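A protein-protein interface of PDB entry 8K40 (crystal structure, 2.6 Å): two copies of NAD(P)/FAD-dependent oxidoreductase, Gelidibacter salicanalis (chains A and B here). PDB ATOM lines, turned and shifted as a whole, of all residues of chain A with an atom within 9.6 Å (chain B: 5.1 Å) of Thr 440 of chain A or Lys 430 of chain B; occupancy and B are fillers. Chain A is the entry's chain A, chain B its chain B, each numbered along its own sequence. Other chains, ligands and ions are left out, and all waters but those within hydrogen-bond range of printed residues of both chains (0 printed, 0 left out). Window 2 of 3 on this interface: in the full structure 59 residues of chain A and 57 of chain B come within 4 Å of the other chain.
The side-chain sulfur (SD) of Met 427 of chain A lies within hydrogen-bond range of the backbone NH (N) of Ala 428 of chain B, 3.8 Å away. The backbone carbonyl oxygen (O) of Asp 437 of chain A lies within hydrogen-bond range of the side-chain amino group (NZ) of Lys 430 of chain B, 3.2 Å away. The side-chain amino group (NZ) of Lys 430 of chain B lies within hydrogen-bond range of the side-chain hydroxyl (OG1) of Thr 440 of chain A (3.4 Å).
The backbone carbonyl oxygen (O) of Ala 428 of chain B sits at hydrogen-bond distance from the side-chain hydroxyl (OG1) of Thr 431 of chain B (3.3 Å). The side-chain hydroxyl of Thr 431 of chain B sits at hydrogen-bond distance from the backbone carbonyl oxygen of Met 427 of chain B, 2.7 Å away. The backbone carbonyl oxygen (O) of Asn 436 of chain A sits close to the side-chain hydroxyl (OG1) of Thr 440 of chain A (3.3 Å). The side-chain hydroxyl of Thr 431 of chain A lies within hydrogen-bond range of the backbone carbonyl oxygen of Met 427 of chain A (2.8 Å).
Thr 440 of chain A touches just these residues of chain B: Pro 345 (3.8 Å) and Lys 430 (3.4 Å). Printed residues of chain A within 4 Å of Lys 430 of chain B: Met 433 (3.999 Å), Asp 437 (3.2 Å), Thr 440 (3.4 Å) and Met 441 (3.9 Å). Of the printed residues of chain A, Pro 346 of chain B touches Ile 442. Of the printed residues of chain B, Ile 442 of chain A touches Pro 345 (3.7 Å) and Pro 346 (3.6 Å). Of the printed residues of chain B, Asp 437 of chain A touches Lys 430 (3.2 Å). Printed residues of chain A within 4 Å of Ala 428 of chain B: Met 427 (3.8 Å). Printed residues of chain A within 4 Å of Met 427 of chain B: Met 427 (3.3 Å), Met 433 (3.7 Å) and Met 441 (3.5 Å). Lys 434 of chain A touches none of the printed residues of chain B. Leu 456 of chain A touches none of the printed residues of chain B. The nearest residue of chain B that does not touch Thr 440 of chain A is Leu 325 of chain B (4.4 Å). The nearest printed residue of chain A that does not touch Lys 430 of chain B is Ile 438 of chain A (5.4 Å). The nearest printed residue of chain B that does not touch Ile 442 of chain A is Leu 325 of chain B (4.1 Å).
Met 427 of chain A touches its own counterpart, Met 427 of chain B. Thr 431 of chain A touches its own counterpart, Thr 431 of chain B. 2 positions are printed for both chains.
Among the printed residues, pairs that only touch across the chains: Met 427 of chain A with Met 427 of chain B (3.3 Å), Met 441 of chain A with Met 427 of chain B (3.5 Å), Ile 442 of chain A with Pro 346 of chain B (3.6 Å), Met 433 of chain A with Thr 431 of chain B (3.7 Å), Met 433 of chain A with Met 427 of chain B (3.7 Å), Thr 431 of chain A with Thr 431 of chain B (3.7 Å), Ile 442 of chain A with Pro 345 of chain B (3.7 Å), Thr 440 of chain A with Pro 345 of chain B (3.8 Å), Met 441 of chain A with Lys 430 of chain B (3.9 Å) and Met 433 of chain A with Lys 430 of chain B (3.999 Å).
Of the 10 printed residues of chain B, 6 touch a printed residue of chain A. Hydrophobic or aromatic side chains of chain B that line the printed part of chain A: Pro 345 and Met 427. Along chain B the printed residues that touch a printed residue of chain A span positions 345 to 431. Hydrophobic or aromatic side chains of chain A within 4 Å of the printed part of chain B: Met 427, Met 433, Met 441 and Ile 442. Among the printed residues, 13 pairs touch across the chains. Among the printed residues, no Asp or Glu carboxylate lies within 4 Å of a Lys or Arg side-chain nitrogen of the other chain.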
ATOM      1  N   MET A 427     -15.966 -36.979   8.611  1.00  0.00           N
ATOM      2  CA  MET A 427     -17.238 -36.214   8.517  1.00  0.00           C
ATOM      3  C   MET A 427     -17.081 -35.172   7.412  1.00  0.00           C
ATOM      4  O   MET A 427     -18.044 -34.954   6.700  1.00  0.00           O
ATOM      5  CB  MET A 427     -17.575 -35.542   9.848  1.00  0.00           C
ATOM      6  CG  MET A 427     -19.001 -35.059   9.962  1.00  0.00           C
ATOM      7  SD  MET A 427     -19.252 -34.132  11.512  1.00  0.00           S
ATOM      8  CE  MET A 427     -19.889 -35.448  12.545  1.00  0.00           C
ATOM      9  N   THR A 431     -19.705 -35.159   4.227  1.00  0.00           N
ATOM     10  CA  THR A 431     -20.546 -33.945   4.064  1.00  0.00           C
ATOM     11  C   THR A 431     -20.025 -33.090   2.900  1.00  0.00           C
ATOM     12  O   THR A 431     -20.625 -32.038   2.634  1.00  0.00           O
ATOM     13  CB  THR A 431     -20.672 -33.171   5.385  1.00  0.00           C
ATOM     14  OG1 THR A 431     -19.395 -32.680   5.781  1.00  0.00           O
ATOM     15  CG2 THR A 431     -21.250 -34.014   6.500  1.00  0.00           C
ATOM     16  N   MET A 433     -17.671 -31.211   2.439  1.00  0.00           N
ATOM     17  CA  MET A 433     -17.335 -29.881   2.987  1.00  0.00           C
ATOM     18  C   MET A 433     -16.148 -29.295   2.214  1.00  0.00           C
ATOM     19  O   MET A 433     -15.123 -29.975   2.101  1.00  0.00           O
ATOM     20  CB  MET A 433     -16.962 -30.084   4.451  1.00  0.00           C
ATOM     21  CG  MET A 433     -17.285 -28.917   5.295  1.00  0.00           C
ATOM     22  SD  MET A 433     -16.875 -29.267   6.996  1.00  0.00           S
ATOM     23  CE  MET A 433     -17.111 -27.625   7.663  1.00  0.00           C
ATOM     24  N   LYS A 434     -16.282 -28.083   1.669  1.00  0.00           N
ATOM     25  CA  LYS A 434     -15.207 -27.412   0.879  1.00  0.00           C
ATOM     26  C   LYS A 434     -14.022 -27.088   1.806  1.00  0.00           C
ATOM     27  O   LYS A 434     -14.230 -26.733   2.997  1.00  0.00           O
ATOM     28  CB  LYS A 434     -15.740 -26.161   0.162  1.00  0.00           C
ATOM     29  CG  LYS A 434     -16.241 -26.373  -1.261  1.00  0.00           C
ATOM     30  CD  LYS A 434     -17.550 -27.124  -1.354  1.00  0.00           C
ATOM     31  CE  LYS A 434     -18.142 -27.154  -2.750  1.00  0.00           C
ATOM     32  NZ  LYS A 434     -17.588 -28.256  -3.573  1.00  0.00           N
ATOM     33  N   VAL A 435     -12.813 -27.203   1.272  1.00  0.00           N
ATOM     34  CA  VAL A 435     -11.544 -26.980   2.014  1.00  0.00           C
ATOM     35  C   VAL A 435     -11.626 -25.629   2.745  1.00  0.00           C
ATOM     36  O   VAL A 435     -11.310 -25.572   3.944  1.00  0.00           O
ATOM     37  CB  VAL A 435     -10.377 -27.087   1.021  1.00  0.00           C
ATOM     38  CG1 VAL A 435      -9.142 -26.336   1.467  1.00  0.00           C
ATOM     39  CG2 VAL A 435     -10.048 -28.540   0.749  1.00  0.00           C
ATOM     40  N   ASN A 436     -12.114 -24.584   2.082  1.00  0.00           N
ATOM     41  CA  ASN A 436     -12.198 -23.227   2.679  1.00  0.00           C
ATOM     42  C   ASN A 436     -13.226 -23.182   3.817  1.00  0.00           C
ATOM     43  O   ASN A 436     -13.112 -22.276   4.656  1.00  0.00           O
ATOM     44  CB  ASN A 436     -12.502 -22.126   1.661  1.00  0.00           C
ATOM     45  CG  ASN A 436     -11.966 -20.803   2.167  1.00  0.00           C
ATOM     46  OD1 ASN A 436     -10.747 -20.616   2.249  1.00  0.00           O
ATOM     47  ND2 ASN A 436     -12.858 -19.920   2.596  1.00  0.00           N
ATOM     48  N   ASP A 437     -14.211 -24.079   3.854  1.00  0.00           N
ATOM     49  CA  ASP A 437     -15.239 -24.058   4.929  1.00  0.00           C
ATOM     50  C   ASP A 437     -14.644 -24.698   6.190  1.00  0.00           C
ATOM     51  O   ASP A 437     -15.169 -24.425   7.280  1.00  0.00           O
ATOM     52  CB  ASP A 437     -16.554 -24.718   4.494  1.00  0.00           C
ATOM     53  CG  ASP A 437     -17.371 -23.909   3.491  1.00  0.00           C
ATOM     54  OD1 ASP A 437     -17.481 -22.671   3.675  1.00  0.00           O
ATOM     55  OD2 ASP A 437     -17.900 -24.528   2.534  1.00  0.00           O
ATOM     56  N   ILE A 438     -13.610 -25.534   6.044  1.00  0.00           N
ATOM     57  CA  ILE A 438     -12.898 -26.173   7.190  1.00  0.00           C
ATOM     58  C   ILE A 438     -11.865 -25.161   7.697  1.00  0.00           C
ATOM     59  O   ILE A 438     -11.671 -25.061   8.928  1.00  0.00           O
ATOM     60  CB  ILE A 438     -12.258 -27.530   6.809  1.00  0.00           C
ATOM     61  CG1 ILE A 438     -13.264 -28.504   6.196  1.00  0.00           C
ATOM     62  CG2 ILE A 438     -11.577 -28.179   8.002  1.00  0.00           C
ATOM     63  CD1 ILE A 438     -12.607 -29.651   5.467  1.00  0.00           C
ATOM     64  N   ARG A 439     -11.219 -24.438   6.788  1.00  0.00           N
ATOM     65  CA  ARG A 439     -10.188 -23.441   7.165  1.00  0.00           C
ATOM     66  C   ARG A 439     -10.816 -22.367   8.063  1.00  0.00           C
ATOM     67  O   ARG A 439     -10.211 -22.070   9.106  1.00  0.00           O
ATOM     68  CB  ARG A 439      -9.527 -22.843   5.922  1.00  0.00           C
ATOM     69  CG  ARG A 439      -8.325 -23.637   5.441  1.00  0.00           C
ATOM     70  CD  ARG A 439      -7.379 -22.792   4.626  1.00  0.00           C
ATOM     71  NE  ARG A 439      -7.597 -23.066   3.215  1.00  0.00           N
ATOM     72  CZ  ARG A 439      -6.917 -23.963   2.505  1.00  0.00           C
ATOM     73  NH1 ARG A 439      -5.946 -24.663   3.070  1.00  0.00           N
ATOM     74  NH2 ARG A 439      -7.193 -24.141   1.222  1.00  0.00           N
ATOM     75  N   THR A 440     -12.008 -21.871   7.724  1.00  0.00           N
ATOM     76  CA  THR A 440     -12.711 -20.767   8.440  1.00  0.00           C
ATOM     77  C   THR A 440     -13.634 -21.262   9.560  1.00  0.00           C
ATOM     78  O   THR A 440     -14.302 -20.398  10.165  1.00  0.00           O
ATOM     79  CB  THR A 440     -13.613 -19.976   7.494  1.00  0.00           C
ATOM     80  OG1 THR A 440     -14.694 -20.840   7.131  1.00  0.00           O
ATOM     81  CG2 THR A 440     -12.861 -19.470   6.287  1.00  0.00           C
ATOM     82  N   MET A 441     -13.724 -22.577   9.792  1.00  0.00           N
ATOM     83  CA  MET A 441     -14.436 -23.153  10.961  1.00  0.00           C
ATOM     84  C   MET A 441     -13.760 -22.708  12.261  1.00  0.00           C
ATOM     85  O   MET A 441     -12.523 -22.435  12.272  1.00  0.00           O
ATOM     86  CB  MET A 441     -14.419 -24.680  10.933  1.00  0.00           C
ATOM     87  CG  MET A 441     -15.770 -25.277  11.069  1.00  0.00           C
ATOM     88  SD  MET A 441     -15.581 -27.053  11.100  1.00  0.00           S
ATOM     89  CE  MET A 441     -15.509 -27.320  12.873  1.00  0.00           C
ATOM     90  N   ILE A 442     -14.547 -22.663  13.331  1.00  0.00           N
ATOM     91  CA  ILE A 442     -14.031 -22.452  14.709  1.00  0.00           C
ATOM     92  C   ILE A 442     -14.023 -23.809  15.415  1.00  0.00           C
ATOM     93  O   ILE A 442     -15.047 -24.540  15.395  1.00  0.00           O
ATOM     94  CB  ILE A 442     -14.817 -21.343  15.435  1.00  0.00           C
ATOM     95  CG1 ILE A 442     -14.322 -19.972  14.956  1.00  0.00           C
ATOM     96  CG2 ILE A 442     -14.728 -21.480  16.947  1.00  0.00           C
ATOM     97  CD1 ILE A 442     -14.984 -18.792  15.632  1.00  0.00           C
ATOM     98  N   PHE A 443     -12.853 -24.135  15.951  1.00  0.00           N
ATOM     99  CA  PHE A 443     -12.582 -25.321  16.784  1.00  0.00           C
ATOM    100  C   PHE A 443     -12.353 -24.846  18.221  1.00  0.00           C
ATOM    101  O   PHE A 443     -11.856 -23.718  18.389  1.00  0.00           O
ATOM    102  CB  PHE A 443     -11.364 -26.041  16.204  1.00  0.00           C
ATOM    103  CG  PHE A 443     -11.607 -26.710  14.877  1.00  0.00           C
ATOM    104  CD1 PHE A 443     -11.536 -25.994  13.691  1.00  0.00           C
ATOM    105  CD2 PHE A 443     -11.957 -28.048  14.819  1.00  0.00           C
ATOM    106  CE1 PHE A 443     -11.794 -26.614  12.477  1.00  0.00           C
ATOM    107  CE2 PHE A 443     -12.222 -28.658  13.606  1.00  0.00           C
ATOM    108  CZ  PHE A 443     -12.141 -27.947  12.437  1.00  0.00           C
ATOM    109  N   ILE A 452      -6.492 -29.017  12.363  1.00  0.00           N
ATOM    110  CA  ILE A 452      -7.035 -29.481  11.052  1.00  0.00           C
ATOM    111  C   ILE A 452      -6.951 -28.365  10.009  1.00  0.00           C
ATOM    112  O   ILE A 452      -6.460 -28.619   8.914  1.00  0.00           O
ATOM    113  CB  ILE A 452      -8.440 -30.077  11.216  1.00  0.00           C
ATOM    114  CG1 ILE A 452      -8.333 -31.483  11.792  1.00  0.00           C
ATOM    115  CG2 ILE A 452      -9.227 -30.077   9.921  1.00  0.00           C
ATOM    116  CD1 ILE A 452      -9.668 -32.103  12.059  1.00  0.00           C
ATOM    117  N   PRO A 453      -7.342 -27.099  10.298  1.00  0.00           N
ATOM    118  CA  PRO A 453      -7.281 -26.032   9.289  1.00  0.00           C
ATOM    119  C   PRO A 453      -5.878 -25.746   8.729  1.00  0.00           C
ATOM    120  O   PRO A 453      -5.764 -25.197   7.640  1.00  0.00           O
ATOM    121  CB  PRO A 453      -7.825 -24.788  10.022  1.00  0.00           C
ATOM    122  CG  PRO A 453      -8.630 -25.344  11.176  1.00  0.00           C
ATOM    123  CD  PRO A 453      -7.913 -26.625  11.571  1.00  0.00           C
ATOM    124  N   HIS A 454      -4.847 -26.125   9.476  1.00  0.00           N
ATOM    125  CA  HIS A 454      -3.425 -25.963   9.090  1.00  0.00           C
ATOM    126  C   HIS A 454      -2.960 -27.183   8.283  1.00  0.00           C
ATOM    127  O   HIS A 454      -1.792 -27.216   7.867  1.00  0.00           O
ATOM    128  CB  HIS A 454      -2.599 -25.684  10.350  1.00  0.00           C
ATOM    129  CG  HIS A 454      -3.069 -24.455  11.051  1.00  0.00           C
ATOM    130  ND1 HIS A 454      -3.767 -24.507  12.259  1.00  0.00           N
ATOM    131  CD2 HIS A 454      -3.011 -23.153  10.686  1.00  0.00           C
ATOM    132  CE1 HIS A 454      -4.082 -23.289  12.627  1.00  0.00           C
ATOM    133  NE2 HIS A 454      -3.640 -22.440  11.666  1.00  0.00           N
ATOM    134  N   LEU A 456      -4.315 -28.269   5.471  1.00  0.00           N
ATOM    135  CA  LEU A 456      -5.005 -28.132   4.171  1.00  0.00           C
ATOM    136  C   LEU A 456      -4.225 -27.138   3.304  1.00  0.00           C
ATOM    137  O   LEU A 456      -4.753 -26.755   2.270  1.00  0.00           O
ATOM    138  CB  LEU A 456      -6.445 -27.694   4.464  1.00  0.00           C
ATOM    139  CG  LEU A 456      -7.284 -28.689   5.267  1.00  0.00           C
ATOM    140  CD1 LEU A 456      -8.629 -28.084   5.624  1.00  0.00           C
ATOM    141  CD2 LEU A 456      -7.476 -29.991   4.495  1.00  0.00           C
ATOM    142  N   LEU B 325     -10.877 -15.091  13.539  1.00  0.00           N
ATOM    143  CA  LEU B 325     -11.967 -14.892  12.553  1.00  0.00           C
ATOM    144  C   LEU B 325     -12.253 -13.390  12.408  1.00  0.00           C
ATOM    145  O   LEU B 325     -12.232 -12.912  11.261  1.00  0.00           O
ATOM    146  CB  LEU B 325     -13.222 -15.649  12.988  1.00  0.00           C
ATOM    147  CG  LEU B 325     -14.396 -15.504  12.026  1.00  0.00           C
ATOM    148  CD1 LEU B 325     -14.040 -16.044  10.643  1.00  0.00           C
ATOM    149  CD2 LEU B 325     -15.623 -16.199  12.583  1.00  0.00           C
ATOM    150  N   PRO B 345     -19.369 -19.124  12.442  1.00  0.00           N
ATOM    151  CA  PRO B 345     -19.724 -20.542  12.462  1.00  0.00           C
ATOM    152  C   PRO B 345     -20.120 -20.912  13.888  1.00  0.00           C
ATOM    153  O   PRO B 345     -20.213 -20.015  14.728  1.00  0.00           O
ATOM    154  CB  PRO B 345     -18.441 -21.255  12.005  1.00  0.00           C
ATOM    155  CG  PRO B 345     -17.326 -20.328  12.463  1.00  0.00           C
ATOM    156  CD  PRO B 345     -17.913 -18.927  12.426  1.00  0.00           C
ATOM    157  N   PRO B 346     -20.424 -22.204  14.188  1.00  0.00           N
ATOM    158  CA  PRO B 346     -20.550 -22.677  15.564  1.00  0.00           C
ATOM    159  C   PRO B 346     -19.269 -22.374  16.352  1.00  0.00           C
ATOM    160  O   PRO B 346     -18.208 -22.412  15.759  1.00  0.00           O
ATOM    161  CB  PRO B 346     -20.757 -24.187  15.405  1.00  0.00           C
ATOM    162  CG  PRO B 346     -21.442 -24.300  14.076  1.00  0.00           C
ATOM    163  CD  PRO B 346     -20.729 -23.269  13.224  1.00  0.00           C
ATOM    164  N   ALA B 426     -19.695 -29.474  16.272  1.00  0.00           N
ATOM    165  CA  ALA B 426     -19.537 -28.192  15.543  1.00  0.00           C
ATOM    166  C   ALA B 426     -19.643 -28.439  14.035  1.00  0.00           C
ATOM    167  O   ALA B 426     -20.398 -27.709  13.373  1.00  0.00           O
ATOM    168  CB  ALA B 426     -18.236 -27.516  15.885  1.00  0.00           C
ATOM    169  N   MET B 427     -18.908 -29.419  13.505  1.00  0.00           N
ATOM    170  CA  MET B 427     -18.926 -29.711  12.049  1.00  0.00           C
ATOM    171  C   MET B 427     -20.358 -30.103  11.677  1.00  0.00           C
ATOM    172  O   MET B 427     -20.836 -29.631  10.634  1.00  0.00           O
ATOM    173  CB  MET B 427     -17.963 -30.835  11.650  1.00  0.00           C
ATOM    174  CG  MET B 427     -16.694 -30.363  10.959  1.00  0.00           C
ATOM    175  SD  MET B 427     -15.782 -31.713  10.135  1.00  0.00           S
ATOM    176  CE  MET B 427     -17.076 -32.288   9.050  1.00  0.00           C
ATOM    177  N   ALA B 428     -21.016 -30.925  12.506  1.00  0.00           N
ATOM    178  CA  ALA B 428     -22.381 -31.436  12.236  1.00  0.00           C
ATOM    179  C   ALA B 428     -23.348 -30.256  12.090  1.00  0.00           C
ATOM    180  O   ALA B 428     -24.182 -30.282  11.154  1.00  0.00           O
ATOM    181  CB  ALA B 428     -22.825 -32.375  13.317  1.00  0.00           C
ATOM    182  N   ILE B 429     -23.207 -29.238  12.943  1.00  0.00           N
ATOM    183  CA  ILE B 429     -24.069 -28.020  12.909  1.00  0.00           C
ATOM    184  C   ILE B 429     -23.752 -27.203  11.648  1.00  0.00           C
ATOM    185  O   ILE B 429     -24.699 -26.892  10.915  1.00  0.00           O
ATOM    186  CB  ILE B 429     -23.929 -27.215  14.215  1.00  0.00           C
ATOM    187  CG1 ILE B 429     -24.415 -28.023  15.424  1.00  0.00           C
ATOM    188  CG2 ILE B 429     -24.642 -25.874  14.114  1.00  0.00           C
ATOM    189  CD1 ILE B 429     -23.911 -27.508  16.766  1.00  0.00           C
ATOM    190  N   LYS B 430     -22.486 -26.875  11.381  1.00  0.00           N
ATOM    191  CA  LYS B 430     -22.096 -26.019  10.227  1.00  0.00           C
ATOM    192  C   LYS B 430     -22.595 -26.669   8.926  1.00  0.00           C
ATOM    193  O   LYS B 430     -23.013 -25.950   8.012  1.00  0.00           O
ATOM    194  CB  LYS B 430     -20.578 -25.783  10.222  1.00  0.00           C
ATOM    195  CG  LYS B 430     -20.024 -25.195   8.929  1.00  0.00           C
ATOM    196  CD  LYS B 430     -18.929 -24.174   9.098  1.00  0.00           C
ATOM    197  CE  LYS B 430     -18.917 -23.182   7.952  1.00  0.00           C
ATOM    198  NZ  LYS B 430     -17.641 -22.431   7.888  1.00  0.00           N
ATOM    199  N   THR B 431     -22.561 -27.992   8.843  1.00  0.00           N
ATOM    200  CA  THR B 431     -22.850 -28.747   7.598  1.00  0.00           C
ATOM    201  C   THR B 431     -24.338 -29.100   7.516  1.00  0.00           C
ATOM    202  O   THR B 431     -24.703 -29.836   6.593  1.00  0.00           O
ATOM    203  CB  THR B 431     -21.944 -29.981   7.512  1.00  0.00           C
ATOM    204  OG1 THR B 431     -22.165 -30.856   8.627  1.00  0.00           O
ATOM    205  CG2 THR B 431     -20.495 -29.563   7.429  1.00  0.00           C
ATOM    206  N   LYS B 432     -25.160 -28.606   8.449  1.00  0.00           N
ATOM    207  CA  LYS B 432     -26.623 -28.880   8.500  1.00  0.00           C
ATOM    208  C   LYS B 432     -26.837 -30.370   8.239  1.00  0.00           C
ATOM    209  O   LYS B 432     -27.720 -30.733   7.435  1.00  0.00           O
ATOM    210  CB  LYS B 432     -27.352 -27.999   7.488  1.00  0.00           C
ATOM    211  CG  LYS B 432     -27.125 -26.512   7.686  1.00  0.00           C
ATOM    212  CD  LYS B 432     -27.923 -25.689   6.721  1.00  0.00           C
ATOM    213  CE  LYS B 432     -27.886 -24.211   7.034  1.00  0.00           C
ATOM    214  NZ  LYS B 432     -28.393 -23.422   5.889  1.00  0.00           N
